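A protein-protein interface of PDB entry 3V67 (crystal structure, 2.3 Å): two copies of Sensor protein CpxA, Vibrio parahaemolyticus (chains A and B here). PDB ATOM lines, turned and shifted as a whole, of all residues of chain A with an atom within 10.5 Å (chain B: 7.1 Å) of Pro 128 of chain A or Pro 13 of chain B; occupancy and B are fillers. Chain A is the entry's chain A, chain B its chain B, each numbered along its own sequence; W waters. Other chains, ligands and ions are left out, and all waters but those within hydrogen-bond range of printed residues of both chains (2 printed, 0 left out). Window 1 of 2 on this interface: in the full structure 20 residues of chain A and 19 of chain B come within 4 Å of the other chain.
A ring nitrogen (NE2) of His 16 of chain B is in hydrogen-bond range of the backbone carbonyl oxygen (O) of Pro 129 of chain A, at 3.5 Å. The backbone carbonyl oxygen (O) of Leu 133 of chain A lies within hydrogen-bond range of the guanidinium group (NE) of Arg 19 of chain B (3.2 Å). The side-chain carboxylate of Glu 127 of chain A lies close to the side-chain carboxylate of Glu 15 of chain B, at 2.8 Å. The guanidinium group (NH1) of Arg 10 of chain A is in salt-bridge range of the side-chain carboxylate (OD2) of Asp 14 of chain B (2.9 Å).
The backbone NH of Gln 96 of chain A lies within hydrogen-bond range of the backbone carbonyl oxygen of Arg 10 of chain A, 2.8 Å away. NE of Arg 101 of chain A is in salt-bridge range of OE2 of Glu 127 of chain A, at 3.9 Å.
Arg 10 of chain A touches Ile 12 of chain B. Pro 13 of chain B touches Pro 128 of chain A. OE2 of Glu 15 of chain B touches CD of Pro 128 of chain A, 3.4 Å away. Pro 128 of chain A touches His 16 of chain B. Pro 130 of chain A touches His 16 of chain B. CD2 of Leu 131 of chain A touches CG of His 16 of chain B (3.5 Å). Phe 123 of chain B touches Leu 131 of chain A (CD2 to CD1, 3.5 Å).
Of chain B, only Pro 13 (3.8 Å), Glu 15 (3.4 Å) and His 16 (3.9 Å) come within 4 Å of Pro 128 of chain A. Of chain A, only Pro 128 (3.8 Å) comes within 4 Å of Pro 13 of chain B. Of chain A, only Arg 10 comes within 4 Å of Ile 12 of chain B. Asp 14 of chain B touches just one residue of chain A: Arg 10 (2.9 Å). Of chain A, only Glu 127 and Pro 128 come within 4 Å of Glu 15 of chain B. Of the printed residues of chain B, Arg 10 of chain A touches Ile 12 and Asp 14. Printed residues of chain A within 4 Å of Phe 123 of chain B: Leu 131. The nearest residue of chain A that does not touch Pro 13 of chain B is Arg 10 of chain A (4.5 Å). The nearest printed residue of chain B that does not touch Pro 130 of chain A is Glu 15 of chain B (6.3 Å).
Of the 15 printed residues of chain B, 7 touch a printed residue of chain A. Hydrophobic or aromatic side chains of chain A within 4 Å of the printed part of chain B: Pro 128, Leu 131 and Leu 133. Among the printed residues, 11 pairs touch across the chains. Among the printed residues, Asp or Glu carboxylates within 4 Å of a Lys or Arg side-chain nitrogen of the other chain: Arg 10 of chain A with Asp 14 of chain B.
Positions printed for both chains: 10, 11, 13, 96, 125 and 127. Of the 11 pairs that touch across the chains among the printed residues, none has its exchanged pair printed and touching as well.
Water W1 lies within hydrogen-bond range of O of Asp 11 of chain A (2.7 Å), OD2 of Asp 11 of chain B (2.7 Å) and NE2 of Gln 96 of chain A (3.4 Å). Water W2 lies within hydrogen-bond range of the side-chain carboxylate (OD2) of Asp 11 of chain B and the backbone NH (N) of Asp 11 of chain A.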
ATOM      1  N   ARG A  10      -6.029  -6.585 -30.388  1.00  0.00           N
ATOM      2  CA  ARG A  10      -5.118  -6.381 -29.274  1.00  0.00           C
ATOM      3  C   ARG A  10      -3.746  -5.954 -29.765  1.00  0.00           C
ATOM      4  O   ARG A  10      -3.375  -6.220 -30.908  1.00  0.00           O
ATOM      5  CB  ARG A  10      -5.015  -7.662 -28.450  1.00  0.00           C
ATOM      6  CG  ARG A  10      -6.365  -8.166 -27.971  1.00  0.00           C
ATOM      7  CD  ARG A  10      -6.309  -9.613 -27.525  1.00  0.00           C
ATOM      8  NE  ARG A  10      -5.442  -9.803 -26.367  1.00  0.00           N
ATOM      9  CZ  ARG A  10      -5.490 -10.865 -25.572  1.00  0.00           C
ATOM     10  NH1 ARG A  10      -6.371 -11.829 -25.806  1.00  0.00           N
ATOM     11  NH2 ARG A  10      -4.665 -10.962 -24.537  1.00  0.00           N
ATOM     12  N   ASP A  11      -3.001  -5.282 -28.895  1.00  0.00           N
ATOM     13  CA  ASP A  11      -1.649  -4.847 -29.216  1.00  0.00           C
ATOM     14  C   ASP A  11      -0.734  -6.038 -29.439  1.00  0.00           C
ATOM     15  O   ASP A  11      -0.883  -7.076 -28.798  1.00  0.00           O
ATOM     16  CB  ASP A  11      -1.082  -3.984 -28.086  1.00  0.00           C
ATOM     17  CG  ASP A  11      -1.612  -2.566 -28.110  1.00  0.00           C
ATOM     18  OD1 ASP A  11      -2.506  -2.273 -28.934  1.00  0.00           O
ATOM     19  OD2 ASP A  11      -1.137  -1.744 -27.298  1.00  0.00           O
ATOM     20  N   PRO A  13       2.817  -7.627 -28.821  1.00  0.00           N
ATOM     21  CA  PRO A  13       3.942  -7.520 -27.886  1.00  0.00           C
ATOM     22  C   PRO A  13       5.165  -6.939 -28.582  1.00  0.00           C
ATOM     23  O   PRO A  13       5.461  -7.339 -29.708  1.00  0.00           O
ATOM     24  CB  PRO A  13       4.204  -8.974 -27.494  1.00  0.00           C
ATOM     25  CG  PRO A  13       2.880  -9.635 -27.630  1.00  0.00           C
ATOM     26  CD  PRO A  13       2.205  -8.967 -28.798  1.00  0.00           C
ATOM     27  N   GLN A  96      -3.268  -7.586 -33.305  1.00  0.00           N
ATOM     28  CA  GLN A  96      -3.400  -9.026 -33.482  1.00  0.00           C
ATOM     29  C   GLN A  96      -4.774  -9.540 -33.059  1.00  0.00           C
ATOM     30  O   GLN A  96      -5.394  -9.003 -32.141  1.00  0.00           O
ATOM     31  CB  GLN A  96      -2.280  -9.782 -32.761  1.00  0.00           C
ATOM     32  CG  GLN A  96      -2.270  -9.616 -31.252  1.00  0.00           C
ATOM     33  CD  GLN A  96      -1.112 -10.351 -30.598  1.00  0.00           C
ATOM     34  OE1 GLN A  96      -0.116 -10.665 -31.249  1.00  0.00           O
ATOM     35  NE2 GLN A  96      -1.240 -10.631 -29.306  1.00  0.00           N
ATOM     36  N   LEU A  98      -7.105 -13.323 -32.424  1.00  0.00           N
ATOM     37  CA  LEU A  98      -7.028 -14.766 -32.232  1.00  0.00           C
ATOM     38  C   LEU A  98      -8.185 -15.492 -32.911  1.00  0.00           C
ATOM     39  O   LEU A  98      -9.352 -15.220 -32.640  1.00  0.00           O
ATOM     40  CB  LEU A  98      -6.983 -15.114 -30.743  1.00  0.00           C
ATOM     41  CG  LEU A  98      -6.708 -16.581 -30.406  1.00  0.00           C
ATOM     42  CD1 LEU A  98      -5.368 -17.020 -30.973  1.00  0.00           C
ATOM     43  CD2 LEU A  98      -6.753 -16.800 -28.901  1.00  0.00           C
ATOM     44  N   GLY A 100      -9.465 -19.067 -33.055  1.00  0.00           N
ATOM     45  CA  GLY A 100      -9.317 -20.367 -32.429  1.00  0.00           C
ATOM     46  C   GLY A 100      -8.006 -20.417 -31.668  1.00  0.00           C
ATOM     47  O   GLY A 100      -7.889 -19.871 -30.573  1.00  0.00           O
ATOM     48  N   ARG A 101      -7.012 -21.065 -32.261  1.00  0.00           N
ATOM     49  CA  ARG A 101      -5.684 -21.138 -31.671  1.00  0.00           C
ATOM     50  C   ARG A 101      -4.667 -20.481 -32.596  1.00  0.00           C
ATOM     51  O   ARG A 101      -3.461 -20.562 -32.362  1.00  0.00           O
ATOM     52  CB  ARG A 101      -5.291 -22.595 -31.415  1.00  0.00           C
ATOM     53  CG  ARG A 101      -6.057 -23.267 -30.283  1.00  0.00           C
ATOM     54  CD  ARG A 101      -5.387 -23.031 -28.937  1.00  0.00           C
ATOM     55  NE  ARG A 101      -6.021 -23.801 -27.868  1.00  0.00           N
ATOM     56  CZ  ARG A 101      -5.726 -25.065 -27.576  1.00  0.00           C
ATOM     57  NH1 ARG A 101      -4.805 -25.712 -28.279  1.00  0.00           N
ATOM     58  NH2 ARG A 101      -6.354 -25.684 -26.586  1.00  0.00           N
ATOM     59  N   MET A 103      -3.237 -17.121 -34.036  1.00  0.00           N
ATOM     60  CA  MET A 103      -3.113 -15.674 -33.918  1.00  0.00           C
ATOM     61  C   MET A 103      -2.641 -15.051 -35.228  1.00  0.00           C
ATOM     62  O   MET A 103      -1.790 -15.606 -35.922  1.00  0.00           O
ATOM     63  CB  MET A 103      -2.127 -15.314 -32.805  1.00  0.00           C
ATOM     64  CG  MET A 103      -2.062 -13.827 -32.496  1.00  0.00           C
ATOM     65  SD  MET A 103      -3.445 -13.292 -31.474  1.00  0.00           S
ATOM     66  CE  MET A 103      -2.934 -13.930 -29.888  1.00  0.00           C
ATOM     67  N   LYS A 124       0.174 -20.180 -34.795  1.00  0.00           N
ATOM     68  CA  LYS A 124      -0.701 -20.796 -33.806  1.00  0.00           C
ATOM     69  C   LYS A 124      -0.284 -20.408 -32.390  1.00  0.00           C
ATOM     70  O   LYS A 124       0.904 -20.327 -32.070  1.00  0.00           O
ATOM     71  CB  LYS A 124      -0.784 -22.316 -33.981  1.00  0.00           C
ATOM     72  CG  LYS A 124       0.359 -23.105 -33.370  1.00  0.00           C
ATOM     73  CD  LYS A 124      -0.175 -24.215 -32.470  1.00  0.00           C
ATOM     74  CE  LYS A 124      -1.163 -25.110 -33.207  1.00  0.00           C
ATOM     75  NZ  LYS A 124      -1.775 -26.121 -32.303  1.00  0.00           N
ATOM     76  N   TRP A 125      -1.281 -20.150 -31.554  1.00  0.00           N
ATOM     77  CA  TRP A 125      -1.049 -19.634 -30.217  1.00  0.00           C
ATOM     78  C   TRP A 125      -1.523 -20.655 -29.189  1.00  0.00           C
ATOM     79  O   TRP A 125      -2.702 -21.008 -29.155  1.00  0.00           O
ATOM     80  CB  TRP A 125      -1.797 -18.314 -30.054  1.00  0.00           C
ATOM     81  CG  TRP A 125      -1.308 -17.481 -28.934  1.00  0.00           C
ATOM     82  CD1 TRP A 125      -0.044 -16.988 -28.772  1.00  0.00           C
ATOM     83  CD2 TRP A 125      -2.063 -17.017 -27.815  1.00  0.00           C
ATOM     84  NE1 TRP A 125       0.038 -16.255 -27.615  1.00  0.00           N
ATOM     85  CE2 TRP A 125      -1.198 -16.246 -27.014  1.00  0.00           C
ATOM     86  CE3 TRP A 125      -3.395 -17.169 -27.415  1.00  0.00           C
ATOM     87  CZ2 TRP A 125      -1.611 -15.647 -25.827  1.00  0.00           C
ATOM     88  CZ3 TRP A 125      -3.805 -16.569 -26.237  1.00  0.00           C
ATOM     89  CH2 TRP A 125      -2.920 -15.815 -25.461  1.00  0.00           C
ATOM     90  N   ASN A 126      -0.603 -21.124 -28.351  1.00  0.00           N
ATOM     91  CA  ASN A 126      -0.879 -22.268 -27.483  1.00  0.00           C
ATOM     92  C   ASN A 126      -1.182 -21.996 -26.018  1.00  0.00           C
ATOM     93  O   ASN A 126      -0.444 -22.449 -25.142  1.00  0.00           O
ATOM     94  CB  ASN A 126       0.234 -23.306 -27.586  1.00  0.00           C
ATOM     95  CG  ASN A 126       0.141 -24.122 -28.847  1.00  0.00           C
ATOM     96  OD1 ASN A 126      -0.918 -24.651 -29.183  1.00  0.00           O
ATOM     97  ND2 ASN A 126       1.249 -24.222 -29.562  1.00  0.00           N
ATOM     98  N   GLU A 127      -2.305 -21.311 -25.795  1.00  0.00           N
ATOM     99  CA  GLU A 127      -3.010 -21.211 -24.508  1.00  0.00           C
ATOM    100  C   GLU A 127      -2.212 -21.604 -23.267  1.00  0.00           C
ATOM    101  O   GLU A 127      -2.001 -22.791 -23.011  1.00  0.00           O
ATOM    102  CB  GLU A 127      -4.306 -22.029 -24.560  1.00  0.00           C
ATOM    103  CG  GLU A 127      -5.283 -21.713 -23.439  1.00  0.00           C
ATOM    104  CD  GLU A 127      -6.626 -21.232 -23.959  1.00  0.00           C
ATOM    105  OE1 GLU A 127      -6.975 -20.057 -23.716  1.00  0.00           O
ATOM    106  OE2 GLU A 127      -7.332 -22.030 -24.612  1.00  0.00           O
ATOM    107  N   PRO A 128      -1.791 -20.602 -22.485  1.00  0.00           N
ATOM    108  CA  PRO A 128      -0.859 -20.749 -21.363  1.00  0.00           C
ATOM    109  C   PRO A 128      -1.334 -21.753 -20.323  1.00  0.00           C
ATOM    110  O   PRO A 128      -2.543 -21.900 -20.128  1.00  0.00           O
ATOM    111  CB  PRO A 128      -0.834 -19.348 -20.745  1.00  0.00           C
ATOM    112  CG  PRO A 128      -1.310 -18.438 -21.818  1.00  0.00           C
ATOM    113  CD  PRO A 128      -2.313 -19.230 -22.589  1.00  0.00           C
ATOM    114  N   PRO A 129      -0.387 -22.439 -19.664  1.00  0.00           N
ATOM    115  CA  PRO A 129      -0.728 -23.317 -18.544  1.00  0.00           C
ATOM    116  C   PRO A 129      -1.460 -22.497 -17.495  1.00  0.00           C
ATOM    117  O   PRO A 129      -0.988 -21.419 -17.130  1.00  0.00           O
ATOM    118  CB  PRO A 129       0.637 -23.773 -18.021  1.00  0.00           C
ATOM    119  CG  PRO A 129       1.619 -22.771 -18.554  1.00  0.00           C
ATOM    120  CD  PRO A 129       1.067 -22.340 -19.872  1.00  0.00           C
ATOM    121  N   PRO A 130      -2.613 -22.992 -17.028  1.00  0.00           N
ATOM    122  CA  PRO A 130      -3.499 -22.204 -16.170  1.00  0.00           C
ATOM    123  C   PRO A 130      -2.869 -21.887 -14.826  1.00  0.00           C
ATOM    124  O   PRO A 130      -1.897 -22.528 -14.424  1.00  0.00           O
ATOM    125  CB  PRO A 130      -4.700 -23.132 -15.970  1.00  0.00           C
ATOM    126  CG  PRO A 130      -4.138 -24.500 -16.131  1.00  0.00           C
ATOM    127  CD  PRO A 130      -3.097 -24.372 -17.204  1.00  0.00           C
ATOM    128  N   LEU A 131      -3.417 -20.887 -14.149  1.00  0.00           N
ATOM    129  CA  LEU A 131      -3.052 -20.630 -12.767  1.00  0.00           C
ATOM    130  C   LEU A 131      -4.301 -20.725 -11.898  1.00  0.00           C
ATOM    131  O   LEU A 131      -5.385 -20.292 -12.293  1.00  0.00           O
ATOM    132  CB  LEU A 131      -2.359 -19.268 -12.613  1.00  0.00           C
ATOM    133  CG  LEU A 131      -3.183 -17.987 -12.438  1.00  0.00           C
ATOM    134  CD1 LEU A 131      -2.271 -16.840 -12.046  1.00  0.00           C
ATOM    135  CD2 LEU A 131      -3.956 -17.641 -13.698  1.00  0.00           C
ATOM    136  N   LEU A 132      -4.146 -21.329 -10.728  1.00  0.00           N
ATOM    137  CA  LEU A 132      -5.225 -21.420  -9.752  1.00  0.00           C
ATOM    138  C   LEU A 132      -4.628 -21.326  -8.347  1.00  0.00           C
ATOM    139  O   LEU A 132      -3.794 -22.158  -7.992  1.00  0.00           O
ATOM    140  CB  LEU A 132      -6.092 -22.680  -9.957  1.00  0.00           C
ATOM    141  CG  LEU A 132      -5.633 -24.153  -9.985  1.00  0.00           C
ATOM    142  CD1 LEU A 132      -4.389 -24.411 -10.844  1.00  0.00           C
ATOM    143  CD2 LEU A 132      -5.471 -24.745  -8.581  1.00  0.00           C
ATOM    144  N   LEU A 133      -5.018 -20.336  -7.532  1.00  0.00           N
ATOM    145  CA  LEU A 133      -6.171 -19.426  -7.703  1.00  0.00           C
ATOM    146  C   LEU A 133      -7.533 -20.119  -7.693  1.00  0.00           C
ATOM    147  O   LEU A 133      -8.251 -20.143  -8.692  1.00  0.00           O
ATOM    148  CB  LEU A 133      -6.029 -18.411  -8.855  1.00  0.00           C
ATOM    149  CG  LEU A 133      -5.268 -17.135  -8.503  1.00  0.00           C
ATOM    150  CD1 LEU A 133      -5.469 -16.072  -9.569  1.00  0.00           C
ATOM    151  CD2 LEU A 133      -5.704 -16.623  -7.139  1.00  0.00           C
ATOM    152  N   ARG B  10       3.850  -6.963 -20.605  1.00  0.00           N
ATOM    153  CA  ARG B  10       3.080  -7.734 -21.567  1.00  0.00           C
ATOM    154  C   ARG B  10       1.642  -7.892 -21.103  1.00  0.00           C
ATOM    155  O   ARG B  10       1.348  -7.793 -19.910  1.00  0.00           O
ATOM    156  CB  ARG B  10       3.733  -9.102 -21.772  1.00  0.00           C
ATOM    157  CG  ARG B  10       5.193  -9.002 -22.187  1.00  0.00           C
ATOM    158  CD  ARG B  10       5.936 -10.308 -21.994  1.00  0.00           C
ATOM    159  NE  ARG B  10       5.411 -11.374 -22.839  1.00  0.00           N
ATOM    160  CZ  ARG B  10       6.076 -12.486 -23.131  1.00  0.00           C
ATOM    161  NH1 ARG B  10       7.299 -12.673 -22.652  1.00  0.00           N
ATOM    162  NH2 ARG B  10       5.523 -13.408 -23.907  1.00  0.00           N
ATOM    163  N   ASP B  11       0.747  -8.125 -22.056  1.00  0.00           N
ATOM    164  CA  ASP B  11      -0.658  -8.351 -21.750  1.00  0.00           C
ATOM    165  C   ASP B  11      -0.843  -9.619 -20.932  1.00  0.00           C
ATOM    166  O   ASP B  11      -0.112 -10.592 -21.100  1.00  0.00           O
ATOM    167  CB  ASP B  11      -1.472  -8.460 -23.040  1.00  0.00           C
ATOM    168  CG  ASP B  11      -1.754  -7.113 -23.669  1.00  0.00           C
ATOM    169  OD1 ASP B  11      -1.225  -6.100 -23.169  1.00  0.00           O
ATOM    170  OD2 ASP B  11      -2.501  -7.069 -24.669  1.00  0.00           O
ATOM    171  N   ILE B  12      -1.824  -9.596 -20.040  1.00  0.00           N
ATOM    172  CA  ILE B  12      -2.222 -10.790 -19.319  1.00  0.00           C
ATOM    173  C   ILE B  12      -3.218 -11.557 -20.178  1.00  0.00           C
ATOM    174  O   ILE B  12      -4.167 -10.970 -20.699  1.00  0.00           O
ATOM    175  CB  ILE B  12      -2.886 -10.434 -17.979  1.00  0.00           C
ATOM    176  CG1 ILE B  12      -2.056  -9.389 -17.228  1.00  0.00           C
ATOM    177  CG2 ILE B  12      -3.086 -11.683 -17.131  1.00  0.00           C
ATOM    178  CD1 ILE B  12      -2.714  -8.869 -15.965  1.00  0.00           C
ATOM    179  N   PRO B  13      -2.990 -12.871 -20.350  1.00  0.00           N
ATOM    180  CA  PRO B  13      -3.913 -13.753 -21.076  1.00  0.00           C
ATOM    181  C   PRO B  13      -5.323 -13.644 -20.511  1.00  0.00           C
ATOM    182  O   PRO B  13      -5.486 -13.625 -19.292  1.00  0.00           O
ATOM    183  CB  PRO B  13      -3.346 -15.145 -20.804  1.00  0.00           C
ATOM    184  CG  PRO B  13      -1.895 -14.917 -20.595  1.00  0.00           C
ATOM    185  CD  PRO B  13      -1.777 -13.584 -19.912  1.00  0.00           C
ATOM    186  N   ASP B  14      -6.317 -13.576 -21.393  1.00  0.00           N
ATOM    187  CA  ASP B  14      -7.700 -13.308 -21.004  1.00  0.00           C
ATOM    188  C   ASP B  14      -8.230 -14.214 -19.895  1.00  0.00           C
ATOM    189  O   ASP B  14      -8.976 -13.764 -19.028  1.00  0.00           O
ATOM    190  CB  ASP B  14      -8.619 -13.378 -22.225  1.00  0.00           C
ATOM    191  CG  ASP B  14      -8.310 -12.304 -23.246  1.00  0.00           C
ATOM    192  OD1 ASP B  14      -7.551 -11.370 -22.914  1.00  0.00           O
ATOM    193  OD2 ASP B  14      -8.833 -12.387 -24.377  1.00  0.00           O
ATOM    194  N   GLU B  15      -7.848 -15.486 -19.931  1.00  0.00           N
ATOM    195  CA  GLU B  15      -8.270 -16.442 -18.914  1.00  0.00           C
ATOM    196  C   GLU B  15      -7.657 -16.094 -17.563  1.00  0.00           C
ATOM    197  O   GLU B  15      -8.331 -16.126 -16.527  1.00  0.00           O
ATOM    198  CB  GLU B  15      -7.897 -17.869 -19.324  1.00  0.00           C
ATOM    199  CG  GLU B  15      -6.469 -18.032 -19.838  1.00  0.00           C
ATOM    200  CD  GLU B  15      -6.349 -17.813 -21.339  1.00  0.00           C
ATOM    201  OE1 GLU B  15      -7.389 -17.832 -22.030  1.00  0.00           O
ATOM    202  OE2 GLU B  15      -5.213 -17.623 -21.826  1.00  0.00           O
ATOM    203  N   HIS B  16      -6.373 -15.751 -17.583  1.00  0.00           N
ATOM    204  CA  HIS B  16      -5.669 -15.354 -16.375  1.00  0.00           C
ATOM    205  C   HIS B  16      -6.255 -14.069 -15.801  1.00  0.00           C
ATOM    206  O   HIS B  16      -6.529 -13.993 -14.611  1.00  0.00           O
ATOM    207  CB  HIS B  16      -4.171 -15.182 -16.652  1.00  0.00           C
ATOM    208  CG  HIS B  16      -3.459 -16.465 -16.955  1.00  0.00           C
ATOM    209  ND1 HIS B  16      -2.097 -16.614 -16.798  1.00  0.00           N
ATOM    210  CD2 HIS B  16      -3.918 -17.657 -17.401  1.00  0.00           C
ATOM    211  CE1 HIS B  16      -1.749 -17.845 -17.132  1.00  0.00           C
ATOM    212  NE2 HIS B  16      -2.837 -18.499 -17.501  1.00  0.00           N
ATOM    213  N   TYR B  17      -6.450 -13.062 -16.648  1.00  0.00           N
ATOM    214  CA  TYR B  17      -7.013 -11.793 -16.195  1.00  0.00           C
ATOM    215  C   TYR B  17      -8.428 -11.962 -15.633  1.00  0.00           C
ATOM    216  O   TYR B  17      -8.756 -11.408 -14.582  1.00  0.00           O
ATOM    217  CB  TYR B  17      -7.001 -10.752 -17.320  1.00  0.00           C
ATOM    218  CG  TYR B  17      -7.732  -9.480 -16.953  1.00  0.00           C
ATOM    219  CD1 TYR B  17      -7.142  -8.527 -16.133  1.00  0.00           C
ATOM    220  CD2 TYR B  17      -9.020  -9.238 -17.413  1.00  0.00           C
ATOM    221  CE1 TYR B  17      -7.811  -7.367 -15.787  1.00  0.00           C
ATOM    222  CE2 TYR B  17      -9.697  -8.080 -17.073  1.00  0.00           C
ATOM    223  CZ  TYR B  17      -9.087  -7.149 -16.261  1.00  0.00           C
ATOM    224  OH  TYR B  17      -9.758  -5.998 -15.922  1.00  0.00           O
ATOM    225  N   GLN B  18      -9.257 -12.727 -16.342  1.00  0.00           N
ATOM    226  CA  GLN B  18     -10.616 -13.032 -15.902  1.00  0.00           C
ATOM    227  C   GLN B  18     -10.599 -13.707 -14.538  1.00  0.00           C
ATOM    228  O   GLN B  18     -11.376 -13.351 -13.641  1.00  0.00           O
ATOM    229  CB  GLN B  18     -11.314 -13.928 -16.929  1.00  0.00           C
ATOM    230  CG  GLN B  18     -12.340 -14.890 -16.355  1.00  0.00           C
ATOM    231  CD  GLN B  18     -13.682 -14.243 -16.090  1.00  0.00           C
ATOM    232  OE1 GLN B  18     -13.812 -13.421 -15.184  1.00  0.00           O
ATOM    233  NE2 GLN B  18     -14.696 -14.624 -16.870  1.00  0.00           N
ATOM    234  N   ARG B  19      -9.691 -14.665 -14.381  1.00  0.00           N
ATOM    235  CA  ARG B  19      -9.509 -15.337 -13.103  1.00  0.00           C
ATOM    236  C   ARG B  19      -9.154 -14.342 -12.002  1.00  0.00           C
ATOM    237  O   ARG B  19      -9.785 -14.326 -10.949  1.00  0.00           O
ATOM    238  CB  ARG B  19      -8.426 -16.411 -13.207  1.00  0.00           C
ATOM    239  CG  ARG B  19      -8.094 -17.057 -11.876  1.00  0.00           C
ATOM    240  CD  ARG B  19      -9.304 -17.770 -11.290  1.00  0.00           C
ATOM    241  NE  ARG B  19      -9.264 -19.207 -11.541  1.00  0.00           N
ATOM    242  CZ  ARG B  19      -9.813 -19.801 -12.594  1.00  0.00           C
ATOM    243  NH1 ARG B  19     -10.454 -19.083 -13.505  1.00  0.00           N
ATOM    244  NH2 ARG B  19      -9.720 -21.116 -12.736  1.00  0.00           N
ATOM    245  N   ILE B  20      -8.144 -13.515 -12.261  1.00  0.00           N
ATOM    246  CA  ILE B  20      -7.702 -12.488 -11.319  1.00  0.00           C
ATOM    247  C   ILE B  20      -8.860 -11.604 -10.866  1.00  0.00           C
ATOM    248  O   ILE B  20      -9.005 -11.312  -9.679  1.00  0.00           O
ATOM    249  CB  ILE B  20      -6.600 -11.606 -11.939  1.00  0.00           C
ATOM    250  CG1 ILE B  20      -5.321 -12.420 -12.139  1.00  0.00           C
ATOM    251  CG2 ILE B  20      -6.316 -10.396 -11.063  1.00  0.00           C
ATOM    252  CD1 ILE B  20      -4.224 -11.667 -12.858  1.00  0.00           C
ATOM    253  N   GLN B  96       1.735  -7.880 -17.175  1.00  0.00           N
ATOM    254  CA  GLN B  96       2.562  -8.830 -16.444  1.00  0.00           C
ATOM    255  C   GLN B  96       4.040  -8.704 -16.811  1.00  0.00           C
ATOM    256  O   GLN B  96       4.382  -8.371 -17.945  1.00  0.00           O
ATOM    257  CB  GLN B  96       2.061 -10.268 -16.634  1.00  0.00           C
ATOM    258  CG  GLN B  96       2.122 -10.786 -18.061  1.00  0.00           C
ATOM    259  CD  GLN B  96       1.578 -12.199 -18.190  1.00  0.00           C
ATOM    260  OE1 GLN B  96       0.828 -12.667 -17.334  1.00  0.00           O
ATOM    261  NE2 GLN B  96       1.957 -12.884 -19.262  1.00  0.00           N
ATOM    262  N   PHE B 123       3.312 -15.593  -9.499  1.00  0.00           N
ATOM    263  CA  PHE B 123       3.263 -17.028  -9.737  1.00  0.00           C
ATOM    264  C   PHE B 123       4.444 -17.436 -10.597  1.00  0.00           C
ATOM    265  O   PHE B 123       4.739 -16.786 -11.595  1.00  0.00           O
ATOM    266  CB  PHE B 123       1.944 -17.428 -10.411  1.00  0.00           C
ATOM    267  CG  PHE B 123       1.618 -16.627 -11.644  1.00  0.00           C
ATOM    268  CD1 PHE B 123       2.004 -17.070 -12.900  1.00  0.00           C
ATOM    269  CD2 PHE B 123       0.913 -15.438 -11.550  1.00  0.00           C
ATOM    270  CE1 PHE B 123       1.701 -16.337 -14.035  1.00  0.00           C
ATOM    271  CE2 PHE B 123       0.608 -14.702 -12.683  1.00  0.00           C
ATOM    272  CZ  PHE B 123       1.003 -15.154 -13.927  1.00  0.00           C
ATOM    273  N   TRP B 125       6.672 -19.117 -13.358  1.00  0.00           N
ATOM    274  CA  TRP B 125       6.347 -19.405 -14.745  1.00  0.00           C
ATOM    275  C   TRP B 125       7.383 -20.360 -15.323  1.00  0.00           C
ATOM    276  O   TRP B 125       8.567 -20.035 -15.383  1.00  0.00           O
ATOM    277  CB  TRP B 125       6.320 -18.099 -15.537  1.00  0.00           C
ATOM    278  CG  TRP B 125       5.580 -18.182 -16.816  1.00  0.00           C
ATOM    279  CD1 TRP B 125       4.269 -18.519 -16.983  1.00  0.00           C
ATOM    280  CD2 TRP B 125       6.095 -17.911 -18.119  1.00  0.00           C
ATOM    281  NE1 TRP B 125       3.937 -18.487 -18.313  1.00  0.00           N
ATOM    282  CE2 TRP B 125       5.037 -18.095 -19.032  1.00  0.00           C
ATOM    283  CE3 TRP B 125       7.343 -17.511 -18.607  1.00  0.00           C
ATOM    284  CZ2 TRP B 125       5.198 -17.926 -20.406  1.00  0.00           C
ATOM    285  CZ3 TRP B 125       7.499 -17.336 -19.969  1.00  0.00           C
ATOM    286  CH2 TRP B 125       6.430 -17.531 -20.851  1.00  0.00           C
ATOM    287  N   GLU B 127       7.808 -21.865 -18.460  1.00  0.00           N
ATOM    288  CA  GLU B 127       7.606 -22.112 -19.882  1.00  0.00           C
ATOM    289  C   GLU B 127       8.053 -20.922 -20.725  1.00  0.00           C
ATOM    290  O   GLU B 127       7.221 -20.207 -21.268  1.00  0.00           O
ATOM    291  CB  GLU B 127       6.125 -22.457 -20.124  1.00  0.00           C
ATOM    292  CG  GLU B 127       5.729 -22.906 -21.534  1.00  0.00           C
ATOM    293  CD  GLU B 127       6.492 -24.126 -22.026  1.00  0.00           C
ATOM    294  OE1 GLU B 127       6.763 -25.041 -21.216  1.00  0.00           O
ATOM    295  OE2 GLU B 127       6.826 -24.162 -23.232  1.00  0.00           O
HETATM  296  O   HOH W   1      -1.369  -8.615 -26.613  1.00  0.00           O
HETATM  297  O   HOH W   2      -4.088  -5.126 -26.169  1.00  0.00           O
